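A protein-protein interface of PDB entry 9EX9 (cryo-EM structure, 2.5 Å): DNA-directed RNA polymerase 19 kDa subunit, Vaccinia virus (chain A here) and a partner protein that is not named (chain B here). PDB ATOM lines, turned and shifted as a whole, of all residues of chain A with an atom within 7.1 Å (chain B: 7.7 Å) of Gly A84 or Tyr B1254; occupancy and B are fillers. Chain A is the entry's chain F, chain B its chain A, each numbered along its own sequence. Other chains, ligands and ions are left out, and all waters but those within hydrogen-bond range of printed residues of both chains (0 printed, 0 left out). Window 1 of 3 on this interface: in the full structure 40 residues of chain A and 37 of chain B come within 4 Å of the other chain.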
ATOM      1  N   LEU A  79      22.100  -5.710  -7.196  1.00  0.00           N
ATOM      2  CA  LEU A  79      22.524  -4.514  -6.479  1.00  0.00           C
ATOM      3  C   LEU A  79      21.635  -3.319  -6.796  1.00  0.00           C
ATOM      4  O   LEU A  79      21.376  -2.488  -5.919  1.00  0.00           O
ATOM      5  CB  LEU A  79      23.976  -4.187  -6.815  1.00  0.00           C
ATOM      6  CG  LEU A  79      25.058  -4.732  -5.889  1.00  0.00           C
ATOM      7  CD1 LEU A  79      26.420  -4.337  -6.408  1.00  0.00           C
ATOM      8  CD2 LEU A  79      24.868  -4.220  -4.480  1.00  0.00           C
ATOM      9  N   PHE A  80      21.174  -3.197  -8.041  1.00  0.00           N
ATOM     10  CA  PHE A  80      20.405  -2.018  -8.424  1.00  0.00           C
ATOM     11  C   PHE A  80      19.152  -1.879  -7.571  1.00  0.00           C
ATOM     12  O   PHE A  80      18.837  -0.790  -7.081  1.00  0.00           O
ATOM     13  CB  PHE A  80      20.035  -2.087  -9.907  1.00  0.00           C
ATOM     14  CG  PHE A  80      21.184  -1.822 -10.845  1.00  0.00           C
ATOM     15  CD1 PHE A  80      22.143  -0.870 -10.552  1.00  0.00           C
ATOM     16  CD2 PHE A  80      21.300  -2.527 -12.026  1.00  0.00           C
ATOM     17  CE1 PHE A  80      23.186  -0.634 -11.414  1.00  0.00           C
ATOM     18  CE2 PHE A  80      22.347  -2.291 -12.887  1.00  0.00           C
ATOM     19  CZ  PHE A  80      23.287  -1.346 -12.579  1.00  0.00           C
ATOM     20  N   GLU A  81      18.436  -2.982  -7.358  1.00  0.00           N
ATOM     21  CA  GLU A  81      17.150  -2.913  -6.672  1.00  0.00           C
ATOM     22  C   GLU A  81      17.321  -2.576  -5.196  1.00  0.00           C
ATOM     23  O   GLU A  81      16.617  -1.712  -4.657  1.00  0.00           O
ATOM     24  CB  GLU A  81      16.415  -4.236  -6.848  1.00  0.00           C
ATOM     25  CG  GLU A  81      16.266  -4.623  -8.302  1.00  0.00           C
ATOM     26  CD  GLU A  81      15.836  -6.049  -8.496  1.00  0.00           C
ATOM     27  OE1 GLU A  81      14.786  -6.432  -7.947  1.00  0.00           O
ATOM     28  OE2 GLU A  81      16.551  -6.788  -9.201  1.00  0.00           O
ATOM     29  N   ILE A  82      18.250  -3.250  -4.521  1.00  0.00           N
ATOM     30  CA  ILE A  82      18.458  -2.984  -3.103  1.00  0.00           C
ATOM     31  C   ILE A  82      19.017  -1.582  -2.904  1.00  0.00           C
ATOM     32  O   ILE A  82      18.654  -0.884  -1.951  1.00  0.00           O
ATOM     33  CB  ILE A  82      19.366  -4.065  -2.487  1.00  0.00           C
ATOM     34  CG1 ILE A  82      19.440  -3.906  -0.969  1.00  0.00           C
ATOM     35  CG2 ILE A  82      20.754  -4.004  -3.075  1.00  0.00           C
ATOM     36  CD1 ILE A  82      18.116  -4.087  -0.269  1.00  0.00           C
ATOM     37  N   ALA A  83      19.894  -1.139  -3.807  1.00  0.00           N
ATOM     38  CA  ALA A  83      20.405   0.223  -3.720  1.00  0.00           C
ATOM     39  C   ALA A  83      19.285   1.239  -3.885  1.00  0.00           C
ATOM     40  O   ALA A  83      19.239   2.242  -3.165  1.00  0.00           O
ATOM     41  CB  ALA A  83      21.494   0.442  -4.768  1.00  0.00           C
ATOM     42  N   GLY A  84      18.362   0.996  -4.816  1.00  0.00           N
ATOM     43  CA  GLY A  84      17.232   1.898  -4.972  1.00  0.00           C
ATOM     44  C   GLY A  84      16.340   1.938  -3.747  1.00  0.00           C
ATOM     45  O   GLY A  84      15.892   3.009  -3.324  1.00  0.00           O
ATOM     46  N   ILE A  85      16.063   0.772  -3.161  1.00  0.00           N
ATOM     47  CA  ILE A  85      15.218   0.724  -1.971  1.00  0.00           C
ATOM     48  C   ILE A  85      15.865   1.499  -0.830  1.00  0.00           C
ATOM     49  O   ILE A  85      15.216   2.306  -0.148  1.00  0.00           O
ATOM     50  CB  ILE A  85      14.939  -0.736  -1.574  1.00  0.00           C
ATOM     51  CG1 ILE A  85      13.985  -1.373  -2.581  1.00  0.00           C
ATOM     52  CG2 ILE A  85      14.375  -0.800  -0.168  1.00  0.00           C
ATOM     53  CD1 ILE A  85      13.759  -2.843  -2.369  1.00  0.00           C
ATOM     54  N   ILE A  86      17.156   1.264  -0.605  1.00  0.00           N
ATOM     55  CA  ILE A  86      17.855   1.977   0.455  1.00  0.00           C
ATOM     56  C   ILE A  86      17.846   3.471   0.179  1.00  0.00           C
ATOM     57  O   ILE A  86      17.687   4.281   1.096  1.00  0.00           O
ATOM     58  CB  ILE A  86      19.287   1.439   0.614  1.00  0.00           C
ATOM     59  CG1 ILE A  86      19.252  -0.008   1.091  1.00  0.00           C
ATOM     60  CG2 ILE A  86      20.063   2.298   1.589  1.00  0.00           C
ATOM     61  CD1 ILE A  86      20.590  -0.674   1.088  1.00  0.00           C
ATOM     62  N   ALA A  87      18.030   3.866  -1.081  1.00  0.00           N
ATOM     63  CA  ALA A  87      18.048   5.286  -1.408  1.00  0.00           C
ATOM     64  C   ALA A  87      16.716   5.939  -1.074  1.00  0.00           C
ATOM     65  O   ALA A  87      16.675   7.009  -0.457  1.00  0.00           O
ATOM     66  CB  ALA A  87      18.383   5.474  -2.884  1.00  0.00           C
ATOM     67  N   GLU A  88      15.612   5.304  -1.469  1.00  0.00           N
ATOM     68  CA  GLU A  88      14.298   5.870  -1.174  1.00  0.00           C
ATOM     69  C   GLU A  88      14.083   5.995   0.326  1.00  0.00           C
ATOM     70  O   GLU A  88      13.665   7.050   0.825  1.00  0.00           O
ATOM     71  CB  GLU A  88      13.201   5.006  -1.789  1.00  0.00           C
ATOM     72  CG  GLU A  88      13.203   4.979  -3.290  1.00  0.00           C
ATOM     73  CD  GLU A  88      12.818   6.305  -3.890  1.00  0.00           C
ATOM     74  OE1 GLU A  88      12.571   7.255  -3.121  1.00  0.00           O
ATOM     75  OE2 GLU A  88      12.762   6.402  -5.131  1.00  0.00           O
ATOM     76  N   SER A  89      14.363   4.918   1.065  1.00  0.00           N
ATOM     77  CA  SER A  89      14.122   4.942   2.502  1.00  0.00           C
ATOM     78  C   SER A  89      14.979   5.999   3.181  1.00  0.00           C
ATOM     79  O   SER A  89      14.500   6.738   4.047  1.00  0.00           O
ATOM     80  CB  SER A  89      14.394   3.565   3.095  1.00  0.00           C
ATOM     81  OG  SER A  89      13.996   3.511   4.451  1.00  0.00           O
ATOM     82  N   TYR A  90      16.250   6.091   2.794  1.00  0.00           N
ATOM     83  CA  TYR A  90      17.150   7.059   3.400  1.00  0.00           C
ATOM     84  C   TYR A  90      16.713   8.483   3.103  1.00  0.00           C
ATOM     85  O   TYR A  90      16.758   9.345   3.982  1.00  0.00           O
ATOM     86  CB  TYR A  90      18.568   6.813   2.899  1.00  0.00           C
ATOM     87  CG  TYR A  90      19.621   7.648   3.568  1.00  0.00           C
ATOM     88  CD1 TYR A  90      19.850   7.547   4.928  1.00  0.00           C
ATOM     89  CD2 TYR A  90      20.408   8.516   2.836  1.00  0.00           C
ATOM     90  CE1 TYR A  90      20.818   8.300   5.540  1.00  0.00           C
ATOM     91  CE2 TYR A  90      21.378   9.274   3.442  1.00  0.00           C
ATOM     92  CZ  TYR A  90      21.581   9.158   4.792  1.00  0.00           C
ATOM     93  OH  TYR A  90      22.549   9.911   5.403  1.00  0.00           O
ATOM     94  N   ILE A 128       8.967   0.627   1.595  1.00  0.00           N
ATOM     95  CA  ILE A 128       9.149   0.796   0.160  1.00  0.00           C
ATOM     96  C   ILE A 128       8.613  -0.420  -0.581  1.00  0.00           C
ATOM     97  O   ILE A 128       8.881  -1.568  -0.207  1.00  0.00           O
ATOM     98  CB  ILE A 128      10.633   1.030  -0.169  1.00  0.00           C
ATOM     99  CG1 ILE A 128      11.208   2.158   0.689  1.00  0.00           C
ATOM    100  CG2 ILE A 128      10.801   1.352  -1.637  1.00  0.00           C
ATOM    101  CD1 ILE A 128      10.502   3.477   0.547  1.00  0.00           C
ATOM    102  N   VAL A 129       7.854  -0.167  -1.645  1.00  0.00           N
ATOM    103  CA  VAL A 129       7.332  -1.203  -2.527  1.00  0.00           C
ATOM    104  C   VAL A 129       7.848  -0.934  -3.932  1.00  0.00           C
ATOM    105  O   VAL A 129       7.820   0.206  -4.404  1.00  0.00           O
ATOM    106  CB  VAL A 129       5.790  -1.244  -2.505  1.00  0.00           C
ATOM    107  CG1 VAL A 129       5.260  -2.089  -3.638  1.00  0.00           C
ATOM    108  CG2 VAL A 129       5.299  -1.779  -1.181  1.00  0.00           C
ATOM    109  N   ILE A 130       8.319  -1.982  -4.597  1.00  0.00           N
ATOM    110  CA  ILE A 130       8.972  -1.873  -5.894  1.00  0.00           C
ATOM    111  C   ILE A 130       8.180  -2.682  -6.906  1.00  0.00           C
ATOM    112  O   ILE A 130       7.646  -3.746  -6.581  1.00  0.00           O
ATOM    113  CB  ILE A 130      10.432  -2.365  -5.830  1.00  0.00           C
ATOM    114  CG1 ILE A 130      11.209  -1.913  -7.058  1.00  0.00           C
ATOM    115  CG2 ILE A 130      10.479  -3.872  -5.740  1.00  0.00           C
ATOM    116  CD1 ILE A 130      12.656  -2.291  -7.009  1.00  0.00           C
ATOM    117  N   GLU A 131       8.097  -2.173  -8.129  1.00  0.00           N
ATOM    118  CA  GLU A 131       7.416  -2.850  -9.224  1.00  0.00           C
ATOM    119  C   GLU A 131       8.467  -3.353 -10.203  1.00  0.00           C
ATOM    120  O   GLU A 131       9.282  -2.566 -10.692  1.00  0.00           O
ATOM    121  CB  GLU A 131       6.438  -1.906  -9.919  1.00  0.00           C
ATOM    122  CG  GLU A 131       5.611  -2.553 -11.002  1.00  0.00           C
ATOM    123  CD  GLU A 131       4.720  -1.564 -11.710  1.00  0.00           C
ATOM    124  OE1 GLU A 131       4.863  -0.353 -11.457  1.00  0.00           O
ATOM    125  OE2 GLU A 131       3.875  -1.993 -12.519  1.00  0.00           O
ATOM    126  N   LYS B 430      19.666  10.489  -2.164  1.00  0.00           N
ATOM    127  CA  LYS B 430      19.689   9.373  -3.102  1.00  0.00           C
ATOM    128  C   LYS B 430      21.019   9.311  -3.834  1.00  0.00           C
ATOM    129  O   LYS B 430      21.610   8.233  -3.989  1.00  0.00           O
ATOM    130  CB  LYS B 430      18.546   9.503  -4.102  1.00  0.00           C
ATOM    131  CG  LYS B 430      17.178   9.477  -3.477  1.00  0.00           C
ATOM    132  CD  LYS B 430      16.101   9.570  -4.527  1.00  0.00           C
ATOM    133  CE  LYS B 430      14.732   9.650  -3.899  1.00  0.00           C
ATOM    134  NZ  LYS B 430      13.670   9.903  -4.904  1.00  0.00           N
ATOM    135  N   ILE B 433      23.671   7.825  -1.512  1.00  0.00           N
ATOM    136  CA  ILE B 433      23.646   6.366  -1.408  1.00  0.00           C
ATOM    137  C   ILE B 433      24.230   5.736  -2.666  1.00  0.00           C
ATOM    138  O   ILE B 433      25.052   4.810  -2.601  1.00  0.00           O
ATOM    139  CB  ILE B 433      22.214   5.870  -1.142  1.00  0.00           C
ATOM    140  CG1 ILE B 433      21.778   6.222   0.279  1.00  0.00           C
ATOM    141  CG2 ILE B 433      22.113   4.375  -1.374  1.00  0.00           C
ATOM    142  CD1 ILE B 433      22.618   5.585   1.369  1.00  0.00           C
ATOM    143  N   GLU B 434      23.823   6.237  -3.831  1.00  0.00           N
ATOM    144  CA  GLU B 434      24.287   5.642  -5.079  1.00  0.00           C
ATOM    145  C   GLU B 434      25.786   5.833  -5.264  1.00  0.00           C
ATOM    146  O   GLU B 434      26.467   4.945  -5.784  1.00  0.00           O
ATOM    147  CB  GLU B 434      23.510   6.225  -6.252  1.00  0.00           C
ATOM    148  CG  GLU B 434      22.054   5.815  -6.249  1.00  0.00           C
ATOM    149  CD  GLU B 434      21.309   6.332  -7.447  1.00  0.00           C
ATOM    150  OE1 GLU B 434      21.837   7.233  -8.126  1.00  0.00           O
ATOM    151  OE2 GLU B 434      20.197   5.836  -7.715  1.00  0.00           O
ATOM    152  N   ILE B 437      27.582   3.227  -3.010  1.00  0.00           N
ATOM    153  CA  ILE B 437      27.530   1.828  -3.422  1.00  0.00           C
ATOM    154  C   ILE B 437      28.031   1.641  -4.849  1.00  0.00           C
ATOM    155  O   ILE B 437      29.002   0.915  -5.083  1.00  0.00           O
ATOM    156  CB  ILE B 437      26.107   1.264  -3.278  1.00  0.00           C
ATOM    157  CG1 ILE B 437      25.689   1.245  -1.808  1.00  0.00           C
ATOM    158  CG2 ILE B 437      26.043  -0.131  -3.862  1.00  0.00           C
ATOM    159  CD1 ILE B 437      24.221   0.976  -1.592  1.00  0.00           C
ATOM    160  N   LEU B 438      27.374   2.284  -5.818  1.00  0.00           N
ATOM    161  CA  LEU B 438      27.580   1.927  -7.220  1.00  0.00           C
ATOM    162  C   LEU B 438      28.889   2.469  -7.785  1.00  0.00           C
ATOM    163  O   LEU B 438      29.534   1.800  -8.599  1.00  0.00           O
ATOM    164  CB  LEU B 438      26.410   2.430  -8.060  1.00  0.00           C
ATOM    165  CG  LEU B 438      25.048   1.825  -7.733  1.00  0.00           C
ATOM    166  CD1 LEU B 438      23.973   2.500  -8.548  1.00  0.00           C
ATOM    167  CD2 LEU B 438      25.039   0.333  -7.986  1.00  0.00           C
ATOM    168  N   VAL B1244      13.864  10.828 -14.420  1.00  0.00           N
ATOM    169  CA  VAL B1244      14.870   9.822 -14.091  1.00  0.00           C
ATOM    170  C   VAL B1244      14.955   8.816 -15.235  1.00  0.00           C
ATOM    171  O   VAL B1244      13.938   8.203 -15.587  1.00  0.00           O
ATOM    172  CB  VAL B1244      14.545   9.132 -12.758  1.00  0.00           C
ATOM    173  CG1 VAL B1244      15.549   8.044 -12.460  1.00  0.00           C
ATOM    174  CG2 VAL B1244      14.532  10.146 -11.634  1.00  0.00           C
ATOM    175  N   GLY B1248      19.535   1.435 -14.733  1.00  0.00           N
ATOM    176  CA  GLY B1248      20.017   1.115 -13.401  1.00  0.00           C
ATOM    177  C   GLY B1248      18.920   1.242 -12.366  1.00  0.00           C
ATOM    178  O   GLY B1248      17.835   0.670 -12.502  1.00  0.00           O
ATOM    179  N   THR B1249      19.201   2.002 -11.307  1.00  0.00           N
ATOM    180  CA  THR B1249      18.230   2.157 -10.231  1.00  0.00           C
ATOM    181  C   THR B1249      16.906   2.700 -10.741  1.00  0.00           C
ATOM    182  O   THR B1249      15.851   2.386 -10.182  1.00  0.00           O
ATOM    183  CB  THR B1249      18.786   3.080  -9.152  1.00  0.00           C
ATOM    184  OG1 THR B1249      19.095   4.354  -9.723  1.00  0.00           O
ATOM    185  CG2 THR B1249      20.036   2.498  -8.548  1.00  0.00           C
ATOM    186  N   GLY B1250      16.936   3.513 -11.789  1.00  0.00           N
ATOM    187  CA  GLY B1250      15.740   4.094 -12.351  1.00  0.00           C
ATOM    188  C   GLY B1250      14.954   3.180 -13.252  1.00  0.00           C
ATOM    189  O   GLY B1250      13.927   3.590 -13.793  1.00  0.00           O
ATOM    190  N   TYR B1251      15.412   1.947 -13.444  1.00  0.00           N
ATOM    191  CA  TYR B1251      14.689   0.997 -14.274  1.00  0.00           C
ATOM    192  C   TYR B1251      13.395   0.520 -13.629  1.00  0.00           C
ATOM    193  O   TYR B1251      12.569  -0.082 -14.321  1.00  0.00           O
ATOM    194  CB  TYR B1251      15.592  -0.194 -14.584  1.00  0.00           C
ATOM    195  CG  TYR B1251      14.979  -1.193 -15.524  1.00  0.00           C
ATOM    196  CD1 TYR B1251      14.903  -0.938 -16.881  1.00  0.00           C
ATOM    197  CD2 TYR B1251      14.483  -2.395 -15.059  1.00  0.00           C
ATOM    198  CE1 TYR B1251      14.345  -1.846 -17.743  1.00  0.00           C
ATOM    199  CE2 TYR B1251      13.923  -3.307 -15.913  1.00  0.00           C
ATOM    200  CZ  TYR B1251      13.857  -3.027 -17.255  1.00  0.00           C
ATOM    201  OH  TYR B1251      13.299  -3.937 -18.116  1.00  0.00           O
ATOM    202  N   TYR B1252      13.192   0.778 -12.342  1.00  0.00           N
ATOM    203  CA  TYR B1252      12.017   0.327 -11.612  1.00  0.00           C
ATOM    204  C   TYR B1252      11.204   1.527 -11.146  1.00  0.00           C
ATOM    205  O   TYR B1252      11.634   2.676 -11.245  1.00  0.00           O
ATOM    206  CB  TYR B1252      12.412  -0.531 -10.409  1.00  0.00           C
ATOM    207  CG  TYR B1252      13.379  -1.630 -10.747  1.00  0.00           C
ATOM    208  CD1 TYR B1252      12.932  -2.867 -11.175  1.00  0.00           C
ATOM    209  CD2 TYR B1252      14.741  -1.430 -10.639  1.00  0.00           C
ATOM    210  CE1 TYR B1252      13.815  -3.868 -11.486  1.00  0.00           C
ATOM    211  CE2 TYR B1252      15.628  -2.424 -10.948  1.00  0.00           C
ATOM    212  CZ  TYR B1252      15.160  -3.640 -11.372  1.00  0.00           C
ATOM    213  OH  TYR B1252      16.051  -4.633 -11.677  1.00  0.00           O
ATOM    214  N   LYS B1253      10.011   1.245 -10.633  1.00  0.00           N
ATOM    215  CA  LYS B1253       9.116   2.264 -10.108  1.00  0.00           C
ATOM    216  C   LYS B1253       8.844   1.981  -8.638  1.00  0.00           C
ATOM    217  O   LYS B1253       8.580   0.837  -8.259  1.00  0.00           O
ATOM    218  CB  LYS B1253       7.809   2.296 -10.898  1.00  0.00           C
ATOM    219  CG  LYS B1253       6.925   3.487 -10.588  1.00  0.00           C
ATOM    220  CD  LYS B1253       5.713   3.527 -11.504  1.00  0.00           C
ATOM    221  CE  LYS B1253       4.690   4.553 -11.043  1.00  0.00           C
ATOM    222  NZ  LYS B1253       5.236   5.936 -11.018  1.00  0.00           N
ATOM    223  N   TYR B1254       8.903   3.024  -7.815  1.00  0.00           N
ATOM    224  CA  TYR B1254       8.858   2.893  -6.365  1.00  0.00           C
ATOM    225  C   TYR B1254       7.595   3.524  -5.794  1.00  0.00           C
ATOM    226  O   TYR B1254       7.162   4.589  -6.243  1.00  0.00           O
ATOM    227  CB  TYR B1254      10.090   3.540  -5.735  1.00  0.00           C
ATOM    228  CG  TYR B1254      11.385   2.971  -6.257  1.00  0.00           C
ATOM    229  CD1 TYR B1254      11.930   1.824  -5.709  1.00  0.00           C
ATOM    230  CD2 TYR B1254      12.055   3.572  -7.309  1.00  0.00           C
ATOM    231  CE1 TYR B1254      13.108   1.296  -6.188  1.00  0.00           C
ATOM    232  CE2 TYR B1254      13.233   3.051  -7.793  1.00  0.00           C
ATOM    233  CZ  TYR B1254      13.754   1.914  -7.228  1.00  0.00           C
ATOM    234  OH  TYR B1254      14.927   1.389  -7.705  1.00  0.00           O
ATOM    235  N   PHE B1255       7.011   2.856  -4.802  1.00  0.00           N
ATOM    236  CA  PHE B1255       5.859   3.347  -4.062  1.00  0.00           C
ATOM    237  C   PHE B1255       6.197   3.344  -2.578  1.00  0.00           C
ATOM    238  O   PHE B1255       7.272   2.906  -2.169  1.00  0.00           O
ATOM    239  CB  PHE B1255       4.617   2.486  -4.311  1.00  0.00           C
ATOM    240  CG  PHE B1255       4.268   2.326  -5.758  1.00  0.00           C
ATOM    241  CD1 PHE B1255       4.924   1.402  -6.540  1.00  0.00           C
ATOM    242  CD2 PHE B1255       3.276   3.091  -6.331  1.00  0.00           C
ATOM    243  CE1 PHE B1255       4.602   1.249  -7.866  1.00  0.00           C
ATOM    244  CE2 PHE B1255       2.952   2.941  -7.656  1.00  0.00           C
ATOM    245  CZ  PHE B1255       3.616   2.020  -8.423  1.00  0.00           C
ATOM    246  N   ILE B1256       5.271   3.837  -1.764  1.00  0.00           N
ATOM    247  CA  ILE B1256       5.405   3.799  -0.313  1.00  0.00           C
ATOM    248  C   ILE B1256       4.124   3.220   0.268  1.00  0.00           C
ATOM    249  O   ILE B1256       3.025   3.657  -0.084  1.00  0.00           O
ATOM    250  CB  ILE B1256       5.697   5.189   0.280  1.00  0.00           C
ATOM    251  CG1 ILE B1256       5.801   5.102   1.802  1.00  0.00           C
ATOM    252  CG2 ILE B1256       4.619   6.177  -0.109  1.00  0.00           C
ATOM    253  CD1 ILE B1256       6.283   6.370   2.448  1.00  0.00           C
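Of chain B, only Tyr B1254 comes within 4 Å of Gly A84.
Of the printed residues of chain A, Tyr B1254 touches Gly A84 (3.6 Å), Glu A88 (3.6 Å), Val A129 (3.5 Å) and Ile A130 (3.7 Å).
Printed residues of chain B within 4 Å of Glu A81: Tyr B1252 (3.3 Å).
Of the printed residues of chain B, Glu A131 touches Tyr B1252, Lys B1253 and Phe B1255.
Of the printed residues of chain A, Phe B1255 touches Ile A128 (3.7 Å), Val A129 (2.8 Å) and Glu A131 (3.9 Å).
The nearest printed residue of chain A that does not touch Tyr B1252 is Phe A80 (4.5 Å).
O of Thr B1249 sits at hydrogen-bond distance from OH of Tyr B1254 (2.8 Å).
The side-chain hydroxyl (OG1) of Thr B1249 sits at hydrogen-bond distance from the side-chain carboxylate (OE2) of Glu B434.
Hydrophobic or aromatic side chains of chain B within 4 Å of the printed part of chain A: Ile B433, Tyr B1252, Tyr B1254 and Phe B1255.
Along chain B the printed residues that touch a printed residue of chain A span positions 430 to 1255.
Of the 16 printed residues of chain A, 10 touch a printed residue of chain B.
Printed residues of chain A that touch a printed residue of chain B: Phe A80, Glu A81, Gly A84, Ala A87, Glu A88, Tyr A90, Ile A128, Val A129, Ile A130 and Glu A131.
Hydrophobic or aromatic side chains of chain A that line the printed part of chain B: Tyr A90, Ile A128 and Ile A130.
Thr B1249 touches Phe A80.
Tyr B1254 touches Gly A84 (OH to CA, 3.6 Å).
Lys B430 touches Ala A87 (CG to O, 3.9 Å).
OE2 of Glu A88 touches CD2 of Tyr B1254 (3.6 Å).
CG1 of Ile B433 touches CD2 of Tyr A90, 3.7 Å away.
Phe B1255 touches Ile A128.
Val A129 touches Tyr B1254 (O to CA, 3.5 Å).
CE1 of Tyr B1254 touches CD1 of Ile A130 (3.7 Å).
O of Glu A131 touches CD1 of Tyr B1252 (3.7 Å).
CE1 of Phe B1255 touches OE1 of Glu A131, at 3.9 Å.
The backbone NH (N) of Phe B1255 lies within hydrogen-bond range of the backbone carbonyl oxygen (O) of Val A129, 2.8 Å away.
NZ of Lys B430 is in salt-bridge range of OE1 of Glu A88, 3.4 Å away.
O of Lys B1253 is in hydrogen-bond range of N of Glu A131, 3.1 Å away.
OH of Tyr B1252 sits at hydrogen-bond distance from OE2 of Glu A81, 3.3 Å away.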
